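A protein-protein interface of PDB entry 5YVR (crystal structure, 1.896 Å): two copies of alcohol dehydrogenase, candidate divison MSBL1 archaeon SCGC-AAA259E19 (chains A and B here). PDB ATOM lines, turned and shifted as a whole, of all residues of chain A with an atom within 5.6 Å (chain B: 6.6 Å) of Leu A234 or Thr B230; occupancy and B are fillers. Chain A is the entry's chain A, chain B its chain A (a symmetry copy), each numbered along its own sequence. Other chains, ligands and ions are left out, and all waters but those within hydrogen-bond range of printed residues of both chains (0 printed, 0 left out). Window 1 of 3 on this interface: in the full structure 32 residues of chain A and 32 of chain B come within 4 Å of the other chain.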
ATOM      1  N   ILE A  21      19.772 -31.997   5.874  1.00  0.00           N
ATOM      2  CA  ILE A  21      20.787 -32.433   6.833  1.00  0.00           C
ATOM      3  C   ILE A  21      20.595 -33.917   7.077  1.00  0.00           C
ATOM      4  O   ILE A  21      19.532 -34.343   7.543  1.00  0.00           O
ATOM      5  CB  ILE A  21      20.693 -31.661   8.162  1.00  0.00           C
ATOM      6  CG1 ILE A  21      20.662 -30.153   7.920  1.00  0.00           C
ATOM      7  CG2 ILE A  21      21.827 -32.138   9.108  1.00  0.00           C
ATOM      8  CD1 ILE A  21      20.432 -29.228   9.239  1.00  0.00           C
ATOM      9  N   VAL A 218      26.556 -19.052  18.995  1.00  0.00           N
ATOM     10  CA  VAL A 218      25.194 -18.895  19.497  1.00  0.00           C
ATOM     11  C   VAL A 218      25.109 -17.781  20.539  1.00  0.00           C
ATOM     12  O   VAL A 218      24.062 -17.106  20.638  1.00  0.00           O
ATOM     13  CB  VAL A 218      24.616 -20.225  20.026  1.00  0.00           C
ATOM     14  CG1 VAL A 218      24.305 -21.161  18.878  1.00  0.00           C
ATOM     15  CG2 VAL A 218      25.516 -20.905  21.113  1.00  0.00           C
ATOM     16  N   THR A 230      13.571 -16.292  15.513  1.00  0.00           N
ATOM     17  CA  THR A 230      13.650 -17.642  14.990  1.00  0.00           C
ATOM     18  C   THR A 230      15.009 -18.284  15.255  1.00  0.00           C
ATOM     19  O   THR A 230      15.114 -19.510  15.196  1.00  0.00           O
ATOM     20  CB  THR A 230      13.358 -17.658  13.468  1.00  0.00           C
ATOM     21  OG1 THR A 230      14.369 -16.914  12.787  1.00  0.00           O
ATOM     22  CG2 THR A 230      12.001 -17.004  13.191  1.00  0.00           C
ATOM     23  N   ALA A 231      16.075 -17.502  15.509  1.00  0.00           N
ATOM     24  CA  ALA A 231      17.337 -18.117  15.874  1.00  0.00           C
ATOM     25  C   ALA A 231      17.413 -18.438  17.361  1.00  0.00           C
ATOM     26  O   ALA A 231      18.082 -19.401  17.727  1.00  0.00           O
ATOM     27  CB  ALA A 231      18.557 -17.247  15.490  1.00  0.00           C
ATOM     28  N   ASP A 232      16.718 -17.689  18.209  1.00  0.00           N
ATOM     29  CA  ASP A 232      17.059 -17.682  19.633  1.00  0.00           C
ATOM     30  C   ASP A 232      16.882 -19.027  20.305  1.00  0.00           C
ATOM     31  O   ASP A 232      17.751 -19.400  21.101  1.00  0.00           O
ATOM     32  CB  ASP A 232      16.227 -16.603  20.349  1.00  0.00           C
ATOM     33  CG  ASP A 232      16.611 -15.198  19.888  1.00  0.00           C
ATOM     34  OD1 ASP A 232      17.682 -15.079  19.226  1.00  0.00           O
ATOM     35  OD2 ASP A 232      15.833 -14.238  20.119  1.00  0.00           O
ATOM     36  N   PRO A 233      15.798 -19.769  20.095  1.00  0.00           N
ATOM     37  CA  PRO A 233      15.678 -21.062  20.783  1.00  0.00           C
ATOM     38  C   PRO A 233      16.740 -22.045  20.365  1.00  0.00           C
ATOM     39  O   PRO A 233      17.172 -22.841  21.199  1.00  0.00           O
ATOM     40  CB  PRO A 233      14.290 -21.565  20.395  1.00  0.00           C
ATOM     41  CG  PRO A 233      13.516 -20.249  19.836  1.00  0.00           C
ATOM     42  CD  PRO A 233      14.616 -19.423  19.277  1.00  0.00           C
ATOM     43  N   LEU A 234      17.109 -22.082  19.073  1.00  0.00           N
ATOM     44  CA  LEU A 234      18.253 -22.906  18.669  1.00  0.00           C
ATOM     45  C   LEU A 234      19.517 -22.463  19.395  1.00  0.00           C
ATOM     46  O   LEU A 234      20.272 -23.295  19.885  1.00  0.00           O
ATOM     47  CB  LEU A 234      18.480 -22.845  17.152  1.00  0.00           C
ATOM     48  CG  LEU A 234      17.171 -23.070  16.344  1.00  0.00           C
ATOM     49  CD1 LEU A 234      17.485 -22.958  14.847  1.00  0.00           C
ATOM     50  CD2 LEU A 234      16.616 -24.443  16.654  1.00  0.00           C
ATOM     51  N   ALA A 235      19.776 -21.162  19.457  1.00  0.00           N
ATOM     52  CA  ALA A 235      21.001 -20.709  20.107  1.00  0.00           C
ATOM     53  C   ALA A 235      21.010 -21.101  21.594  1.00  0.00           C
ATOM     54  O   ALA A 235      22.038 -21.564  22.121  1.00  0.00           O
ATOM     55  CB  ALA A 235      21.152 -19.187  19.970  1.00  0.00           C
ATOM     56  N   ILE A 236      19.872 -20.937  22.275  1.00  0.00           N
ATOM     57  CA  ILE A 236      19.823 -21.236  23.720  1.00  0.00           C
ATOM     58  C   ILE A 236      20.113 -22.715  23.959  1.00  0.00           C
ATOM     59  O   ILE A 236      20.949 -23.088  24.798  1.00  0.00           O
ATOM     60  CB  ILE A 236      18.453 -20.854  24.325  1.00  0.00           C
ATOM     61  CG1 ILE A 236      18.246 -19.345  24.428  1.00  0.00           C
ATOM     62  CG2 ILE A 236      18.246 -21.515  25.700  1.00  0.00           C
ATOM     63  CD1 ILE A 236      19.198 -18.677  25.329  1.00  0.00           C
ATOM     64  N   ARG A 237      19.368 -23.582  23.263  1.00  0.00           N
ATOM     65  CA  ARG A 237      19.551 -25.017  23.432  1.00  0.00           C
ATOM     66  C   ARG A 237      21.014 -25.428  23.187  1.00  0.00           C
ATOM     67  O   ARG A 237      21.558 -26.326  23.862  1.00  0.00           O
ATOM     68  CB  ARG A 237      18.609 -25.735  22.459  1.00  0.00           C
ATOM     69  CG  ARG A 237      18.509 -27.213  22.668  1.00  0.00           C
ATOM     70  CD  ARG A 237      17.887 -27.460  24.070  1.00  0.00           C
ATOM     71  NE  ARG A 237      17.415 -28.818  24.255  1.00  0.00           N
ATOM     72  CZ  ARG A 237      17.215 -29.361  25.457  1.00  0.00           C
ATOM     73  NH1 ARG A 237      16.802 -30.621  25.569  1.00  0.00           N
ATOM     74  NH2 ARG A 237      17.436 -28.635  26.546  1.00  0.00           N
ATOM     75  N   ALA A 238      21.673 -24.772  22.225  1.00  0.00           N
ATOM     76  CA  ALA A 238      23.074 -25.090  21.951  1.00  0.00           C
ATOM     77  C   ALA A 238      23.946 -24.796  23.166  1.00  0.00           C
ATOM     78  O   ALA A 238      24.879 -25.548  23.467  1.00  0.00           O
ATOM     79  CB  ALA A 238      23.588 -24.286  20.761  1.00  0.00           C
ATOM     80  N   ILE A 239      23.695 -23.680  23.837  1.00  0.00           N
ATOM     81  CA  ILE A 239      24.491 -23.390  25.024  1.00  0.00           C
ATOM     82  C   ILE A 239      24.212 -24.420  26.106  1.00  0.00           C
ATOM     83  O   ILE A 239      25.132 -24.831  26.823  1.00  0.00           O
ATOM     84  CB  ILE A 239      24.253 -21.950  25.525  1.00  0.00           C
ATOM     85  CG1 ILE A 239      24.552 -20.933  24.418  1.00  0.00           C
ATOM     86  CG2 ILE A 239      25.186 -21.606  26.715  1.00  0.00           C
ATOM     87  CD1 ILE A 239      24.182 -19.517  24.889  1.00  0.00           C
ATOM     88  N   THR A 267      25.039 -27.861  14.673  1.00  0.00           N
ATOM     89  CA  THR A 267      24.029 -27.629  13.620  1.00  0.00           C
ATOM     90  C   THR A 267      23.115 -26.464  13.987  1.00  0.00           C
ATOM     91  O   THR A 267      22.816 -25.594  13.137  1.00  0.00           O
ATOM     92  CB  THR A 267      23.266 -28.929  13.372  1.00  0.00           C
ATOM     93  OG1 THR A 267      24.191 -29.914  12.878  1.00  0.00           O
ATOM     94  CG2 THR A 267      22.119 -28.745  12.283  1.00  0.00           C
ATOM     95  N   TYR A 268      22.710 -26.396  15.261  1.00  0.00           N
ATOM     96  CA  TYR A 268      21.932 -25.262  15.744  1.00  0.00           C
ATOM     97  C   TYR A 268      22.667 -23.994  15.434  1.00  0.00           C
ATOM     98  O   TYR A 268      22.070 -22.994  14.987  1.00  0.00           O
ATOM     99  CB  TYR A 268      21.717 -25.333  17.277  1.00  0.00           C
ATOM    100  CG  TYR A 268      20.728 -26.356  17.769  1.00  0.00           C
ATOM    101  CD1 TYR A 268      19.747 -26.884  16.925  1.00  0.00           C
ATOM    102  CD2 TYR A 268      20.764 -26.795  19.094  1.00  0.00           C
ATOM    103  CE1 TYR A 268      18.842 -27.834  17.389  1.00  0.00           C
ATOM    104  CE2 TYR A 268      19.846 -27.710  19.570  1.00  0.00           C
ATOM    105  CZ  TYR A 268      18.883 -28.220  18.720  1.00  0.00           C
ATOM    106  OH  TYR A 268      18.027 -29.171  19.208  1.00  0.00           O
ATOM    107  N   LEU A 271      22.580 -22.893  11.737  1.00  0.00           N
ATOM    108  CA  LEU A 271      21.275 -22.333  11.387  1.00  0.00           C
ATOM    109  C   LEU A 271      21.076 -20.981  12.064  1.00  0.00           C
ATOM    110  O   LEU A 271      20.624 -19.997  11.437  1.00  0.00           O
ATOM    111  CB  LEU A 271      20.150 -23.312  11.775  1.00  0.00           C
ATOM    112  CG  LEU A 271      20.261 -24.674  11.079  1.00  0.00           C
ATOM    113  CD1 LEU A 271      19.229 -25.706  11.668  1.00  0.00           C
ATOM    114  CD2 LEU A 271      20.019 -24.463   9.562  1.00  0.00           C
ATOM    115  N   SER A 272      21.435 -20.906  13.359  1.00  0.00           N
ATOM    116  CA  SER A 272      21.288 -19.651  14.098  1.00  0.00           C
ATOM    117  C   SER A 272      22.183 -18.548  13.522  1.00  0.00           C
ATOM    118  O   SER A 272      21.776 -17.375  13.427  1.00  0.00           O
ATOM    119  CB  SER A 272      21.634 -19.894  15.590  1.00  0.00           C
ATOM    120  OG  SER A 272      21.780 -18.678  16.202  1.00  0.00           O
ATOM    121  N   ILE A 275      20.597 -17.144  10.282  1.00  0.00           N
ATOM    122  CA  ILE A 275      19.459 -16.243  10.491  1.00  0.00           C
ATOM    123  C   ILE A 275      19.919 -14.941  11.137  1.00  0.00           C
ATOM    124  O   ILE A 275      19.473 -13.860  10.746  1.00  0.00           O
ATOM    125  CB  ILE A 275      18.369 -16.920  11.350  1.00  0.00           C
ATOM    126  CG1 ILE A 275      17.732 -18.115  10.646  1.00  0.00           C
ATOM    127  CG2 ILE A 275      17.312 -15.876  11.863  1.00  0.00           C
ATOM    128  CD1 ILE A 275      17.264 -19.177  11.688  1.00  0.00           C
ATOM    129  N   PHE B  12      18.543 -38.978  12.004  1.00  0.00           N
ATOM    130  CA  PHE B  12      17.411 -38.282  11.390  1.00  0.00           C
ATOM    131  C   PHE B  12      17.864 -37.607  10.113  1.00  0.00           C
ATOM    132  O   PHE B  12      19.061 -37.444   9.861  1.00  0.00           O
ATOM    133  CB  PHE B  12      16.792 -37.224  12.311  1.00  0.00           C
ATOM    134  CG  PHE B  12      17.745 -36.133  12.705  1.00  0.00           C
ATOM    135  CD1 PHE B  12      18.660 -36.334  13.749  1.00  0.00           C
ATOM    136  CD2 PHE B  12      17.760 -34.929  12.022  1.00  0.00           C
ATOM    137  CE1 PHE B  12      19.570 -35.357  14.117  1.00  0.00           C
ATOM    138  CE2 PHE B  12      18.665 -33.930  12.376  1.00  0.00           C
ATOM    139  CZ  PHE B  12      19.566 -34.141  13.457  1.00  0.00           C
ATOM    140  N   HIS B  14      16.802 -33.941   8.269  1.00  0.00           N
ATOM    141  CA  HIS B  14      16.111 -32.675   8.405  1.00  0.00           C
ATOM    142  C   HIS B  14      15.962 -32.106   7.013  1.00  0.00           C
ATOM    143  O   HIS B  14      16.950 -32.049   6.268  1.00  0.00           O
ATOM    144  CB  HIS B  14      16.922 -31.743   9.285  1.00  0.00           C
ATOM    145  CG  HIS B  14      16.695 -30.289   9.062  1.00  0.00           C
ATOM    146  ND1 HIS B  14      16.195 -29.468  10.056  1.00  0.00           N
ATOM    147  CD2 HIS B  14      17.035 -29.472   8.028  1.00  0.00           C
ATOM    148  CE1 HIS B  14      16.171 -28.219   9.617  1.00  0.00           C
ATOM    149  NE2 HIS B  14      16.678 -28.198   8.388  1.00  0.00           N
ATOM    150  N   ASN B  15      14.741 -31.703   6.675  1.00  0.00           N
ATOM    151  CA  ASN B  15      14.445 -31.053   5.394  1.00  0.00           C
ATOM    152  C   ASN B  15      13.583 -29.832   5.637  1.00  0.00           C
ATOM    153  O   ASN B  15      12.468 -29.954   6.138  1.00  0.00           O
ATOM    154  CB  ASN B  15      13.744 -32.007   4.424  1.00  0.00           C
ATOM    155  CG  ASN B  15      14.679 -33.082   3.935  1.00  0.00           C
ATOM    156  OD1 ASN B  15      14.594 -34.218   4.395  1.00  0.00           O
ATOM    157  ND2 ASN B  15      15.608 -32.726   3.019  1.00  0.00           N
ATOM    158  N   ASP B 227      13.708 -39.205  16.167  1.00  0.00           N
ATOM    159  CA  ASP B 227      14.415 -37.991  16.543  1.00  0.00           C
ATOM    160  C   ASP B 227      14.152 -36.874  15.548  1.00  0.00           C
ATOM    161  O   ASP B 227      14.196 -37.103  14.341  1.00  0.00           O
ATOM    162  CB  ASP B 227      15.908 -38.263  16.584  1.00  0.00           C
ATOM    163  CG  ASP B 227      16.273 -39.260  17.685  1.00  0.00           C
ATOM    164  OD1 ASP B 227      15.746 -39.070  18.803  1.00  0.00           O
ATOM    165  OD2 ASP B 227      16.992 -40.231  17.397  1.00  0.00           O
ATOM    166  N   HIS B 228      13.970 -35.648  16.061  1.00  0.00           N
ATOM    167  CA  HIS B 228      13.796 -34.458  15.215  1.00  0.00           C
ATOM    168  C   HIS B 228      14.311 -33.250  15.999  1.00  0.00           C
ATOM    169  O   HIS B 228      13.553 -32.329  16.322  1.00  0.00           O
ATOM    170  CB  HIS B 228      12.325 -34.277  14.799  1.00  0.00           C
ATOM    171  CG  HIS B 228      11.349 -34.856  15.790  1.00  0.00           C
ATOM    172  ND1 HIS B 228      11.070 -34.257  17.003  1.00  0.00           N
ATOM    173  CD2 HIS B 228      10.634 -36.005  15.770  1.00  0.00           C
ATOM    174  CE1 HIS B 228      10.195 -34.990  17.676  1.00  0.00           C
ATOM    175  NE2 HIS B 228       9.917 -36.063  16.953  1.00  0.00           N
ATOM    176  N   PRO B 229      15.602 -33.208  16.320  1.00  0.00           N
ATOM    177  CA  PRO B 229      16.066 -32.189  17.276  1.00  0.00           C
ATOM    178  C   PRO B 229      16.067 -30.782  16.709  1.00  0.00           C
ATOM    179  O   PRO B 229      16.069 -29.822  17.489  1.00  0.00           O
ATOM    180  CB  PRO B 229      17.479 -32.665  17.653  1.00  0.00           C
ATOM    181  CG  PRO B 229      17.905 -33.486  16.510  1.00  0.00           C
ATOM    182  CD  PRO B 229      16.675 -34.130  15.921  1.00  0.00           C
ATOM    183  N   THR B 230      16.049 -30.594  15.379  1.00  0.00           N
ATOM    184  CA  THR B 230      16.016 -29.226  14.898  1.00  0.00           C
ATOM    185  C   THR B 230      14.638 -28.592  15.058  1.00  0.00           C
ATOM    186  O   THR B 230      14.536 -27.365  15.033  1.00  0.00           O
ATOM    187  CB  THR B 230      16.447 -29.158  13.411  1.00  0.00           C
ATOM    188  OG1 THR B 230      15.505 -29.877  12.614  1.00  0.00           O
ATOM    189  CG2 THR B 230      17.826 -29.804  13.238  1.00  0.00           C
ATOM    190  N   ALA B 231      13.554 -29.380  15.185  1.00  0.00           N
ATOM    191  CA  ALA B 231      12.262 -28.776  15.453  1.00  0.00           C
ATOM    192  C   ALA B 231      12.049 -28.507  16.937  1.00  0.00           C
ATOM    193  O   ALA B 231      11.347 -27.556  17.274  1.00  0.00           O
ATOM    194  CB  ALA B 231      11.084 -29.631  14.929  1.00  0.00           C
ATOM    195  N   ASP B 232      12.664 -29.286  17.820  1.00  0.00           N
ATOM    196  CA  ASP B 232      12.193 -29.343  19.205  1.00  0.00           C
ATOM    197  C   ASP B 232      12.305 -28.022  19.937  1.00  0.00           C
ATOM    198  O   ASP B 232      11.365 -27.675  20.662  1.00  0.00           O
ATOM    199  CB  ASP B 232      12.957 -30.447  19.957  1.00  0.00           C
ATOM    200  CG  ASP B 232      12.619 -31.835  19.414  1.00  0.00           C
ATOM    201  OD1 ASP B 232      11.614 -31.929  18.652  1.00  0.00           O
ATOM    202  OD2 ASP B 232      13.374 -32.803  19.682  1.00  0.00           O
ATOM    203  N   PRO B 233      13.403 -27.275  19.854  1.00  0.00           N
ATOM    204  CA  PRO B 233      13.457 -26.007  20.594  1.00  0.00           C
ATOM    205  C   PRO B 233      12.436 -25.008  20.115  1.00  0.00           C
ATOM    206  O   PRO B 233      11.928 -24.241  20.932  1.00  0.00           O
ATOM    207  CB  PRO B 233      14.874 -25.492  20.353  1.00  0.00           C
ATOM    208  CG  PRO B 233      15.698 -26.789  19.823  1.00  0.00           C
ATOM    209  CD  PRO B 233      14.656 -27.594  19.137  1.00  0.00           C
ATOM    210  N   LEU B 234      12.188 -24.926  18.796  1.00  0.00           N
ATOM    211  CA  LEU B 234      11.085 -24.086  18.317  1.00  0.00           C
ATOM    212  C   LEU B 234       9.760 -24.552  18.907  1.00  0.00           C
ATOM    213  O   LEU B 234       8.962 -23.736  19.354  1.00  0.00           O
ATOM    214  CB  LEU B 234      10.999 -24.095  16.784  1.00  0.00           C
ATOM    215  CG  LEU B 234      12.377 -23.843  16.108  1.00  0.00           C
ATOM    216  CD1 LEU B 234      12.202 -23.903  14.586  1.00  0.00           C
ATOM    217  CD2 LEU B 234      12.898 -22.483  16.516  1.00  0.00           C
ATOM    218  N   ALA B 235       9.499 -25.854  18.900  1.00  0.00           N
ATOM    219  CA  ALA B 235       8.219 -26.328  19.418  1.00  0.00           C
ATOM    220  C   ALA B 235       8.073 -25.987  20.910  1.00  0.00           C
ATOM    221  O   ALA B 235       6.999 -25.541  21.356  1.00  0.00           O
ATOM    222  CB  ALA B 235       8.084 -27.843  19.214  1.00  0.00           C
ATOM    223  N   SER B 272       8.410 -25.895  12.669  1.00  0.00           N
ATOM    224  CA  SER B 272       8.490 -27.176  13.374  1.00  0.00           C
ATOM    225  C   SER B 272       7.654 -28.256  12.680  1.00  0.00           C
ATOM    226  O   SER B 272       8.070 -29.426  12.583  1.00  0.00           O
ATOM    227  CB  SER B 272       8.008 -26.984  14.836  1.00  0.00           C
ATOM    228  OG  SER B 272       7.807 -28.221  15.389  1.00  0.00           O
ATOM    229  N   ILE B 275       9.535 -29.549   9.554  1.00  0.00           N
ATOM    230  CA  ILE B 275      10.650 -30.459   9.836  1.00  0.00           C
ATOM    231  C   ILE B 275      10.134 -31.782  10.391  1.00  0.00           C
ATOM    232  O   ILE B 275      10.616 -32.850  10.006  1.00  0.00           O
ATOM    233  CB  ILE B 275      11.655 -29.815  10.815  1.00  0.00           C
ATOM    234  CG1 ILE B 275      12.353 -28.597  10.214  1.00  0.00           C
ATOM    235  CG2 ILE B 275      12.662 -30.877  11.386  1.00  0.00           C
ATOM    236  CD1 ILE B 275      12.720 -27.572  11.332  1.00  0.00           C
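N of Ile A21 sits at hydrogen-bond distance from O of His B14, at 2.8 Å. The backbone carbonyl oxygen (O) of Pro B229 sits at hydrogen-bond distance from the side-chain hydroxyl (OH) of Tyr A268, at 2.7 Å.
ND1 of His B14 sits at hydrogen-bond distance from OG1 of Thr B230 (2.7 Å).
Among the printed residues, pairs that only touch across the chains: Ile A21 with Phe B12 (3.9 Å), Thr A230 with Leu B234 (3.9 Å), Pro A233 with Pro B233 (3.6 Å), Leu A234 with Thr B230 (3.9 Å) and Tyr A268 with Pro B233 (3.4 Å).
Of the printed residues of chain B, Pro A233 touches Pro B233. Leu A234 touches just one residue of chain B: Thr B230. Of the printed residues of chain A, His B14 touches Ile A21. Of the printed residues of chain A, Thr B230 touches Leu A234 (3.9 Å). Of the printed residues of chain A, Pro B233 touches Pro A233 and Tyr A268. Ser B272 touches none of the printed residues of chain A. The nearest residue of chain B that does not touch Leu A234 is Pro B233 (4.05 Å). The nearest printed residue of chain A that does not touch Thr B230 is Tyr A268 (4.02 Å).
Of the 17 printed residues of chain A, 5 touch a printed residue of chain B. Printed residues of chain A that touch a printed residue of chain B: Ile A21, Thr A230, Pro A233, Leu A234 and Tyr A268. Hydrophobic or aromatic side chains of chain A within 4 Å of the printed part of chain B: Ile A21, Pro A233, Leu A234 and Tyr A268. Of the 14 printed residues of chain B, 6 touch a printed residue of chain A. Among the printed residues, 7 pairs touch across the chains.
Thr A230 touches Leu B234, and with the chains exchanged Leu A234 touches Thr B230. Pro B233 touches its own counterpart, Pro A233. Of the 7 pairs that touch across the chains among the printed residues, 3 have their exchanged pair printed and touching as well.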
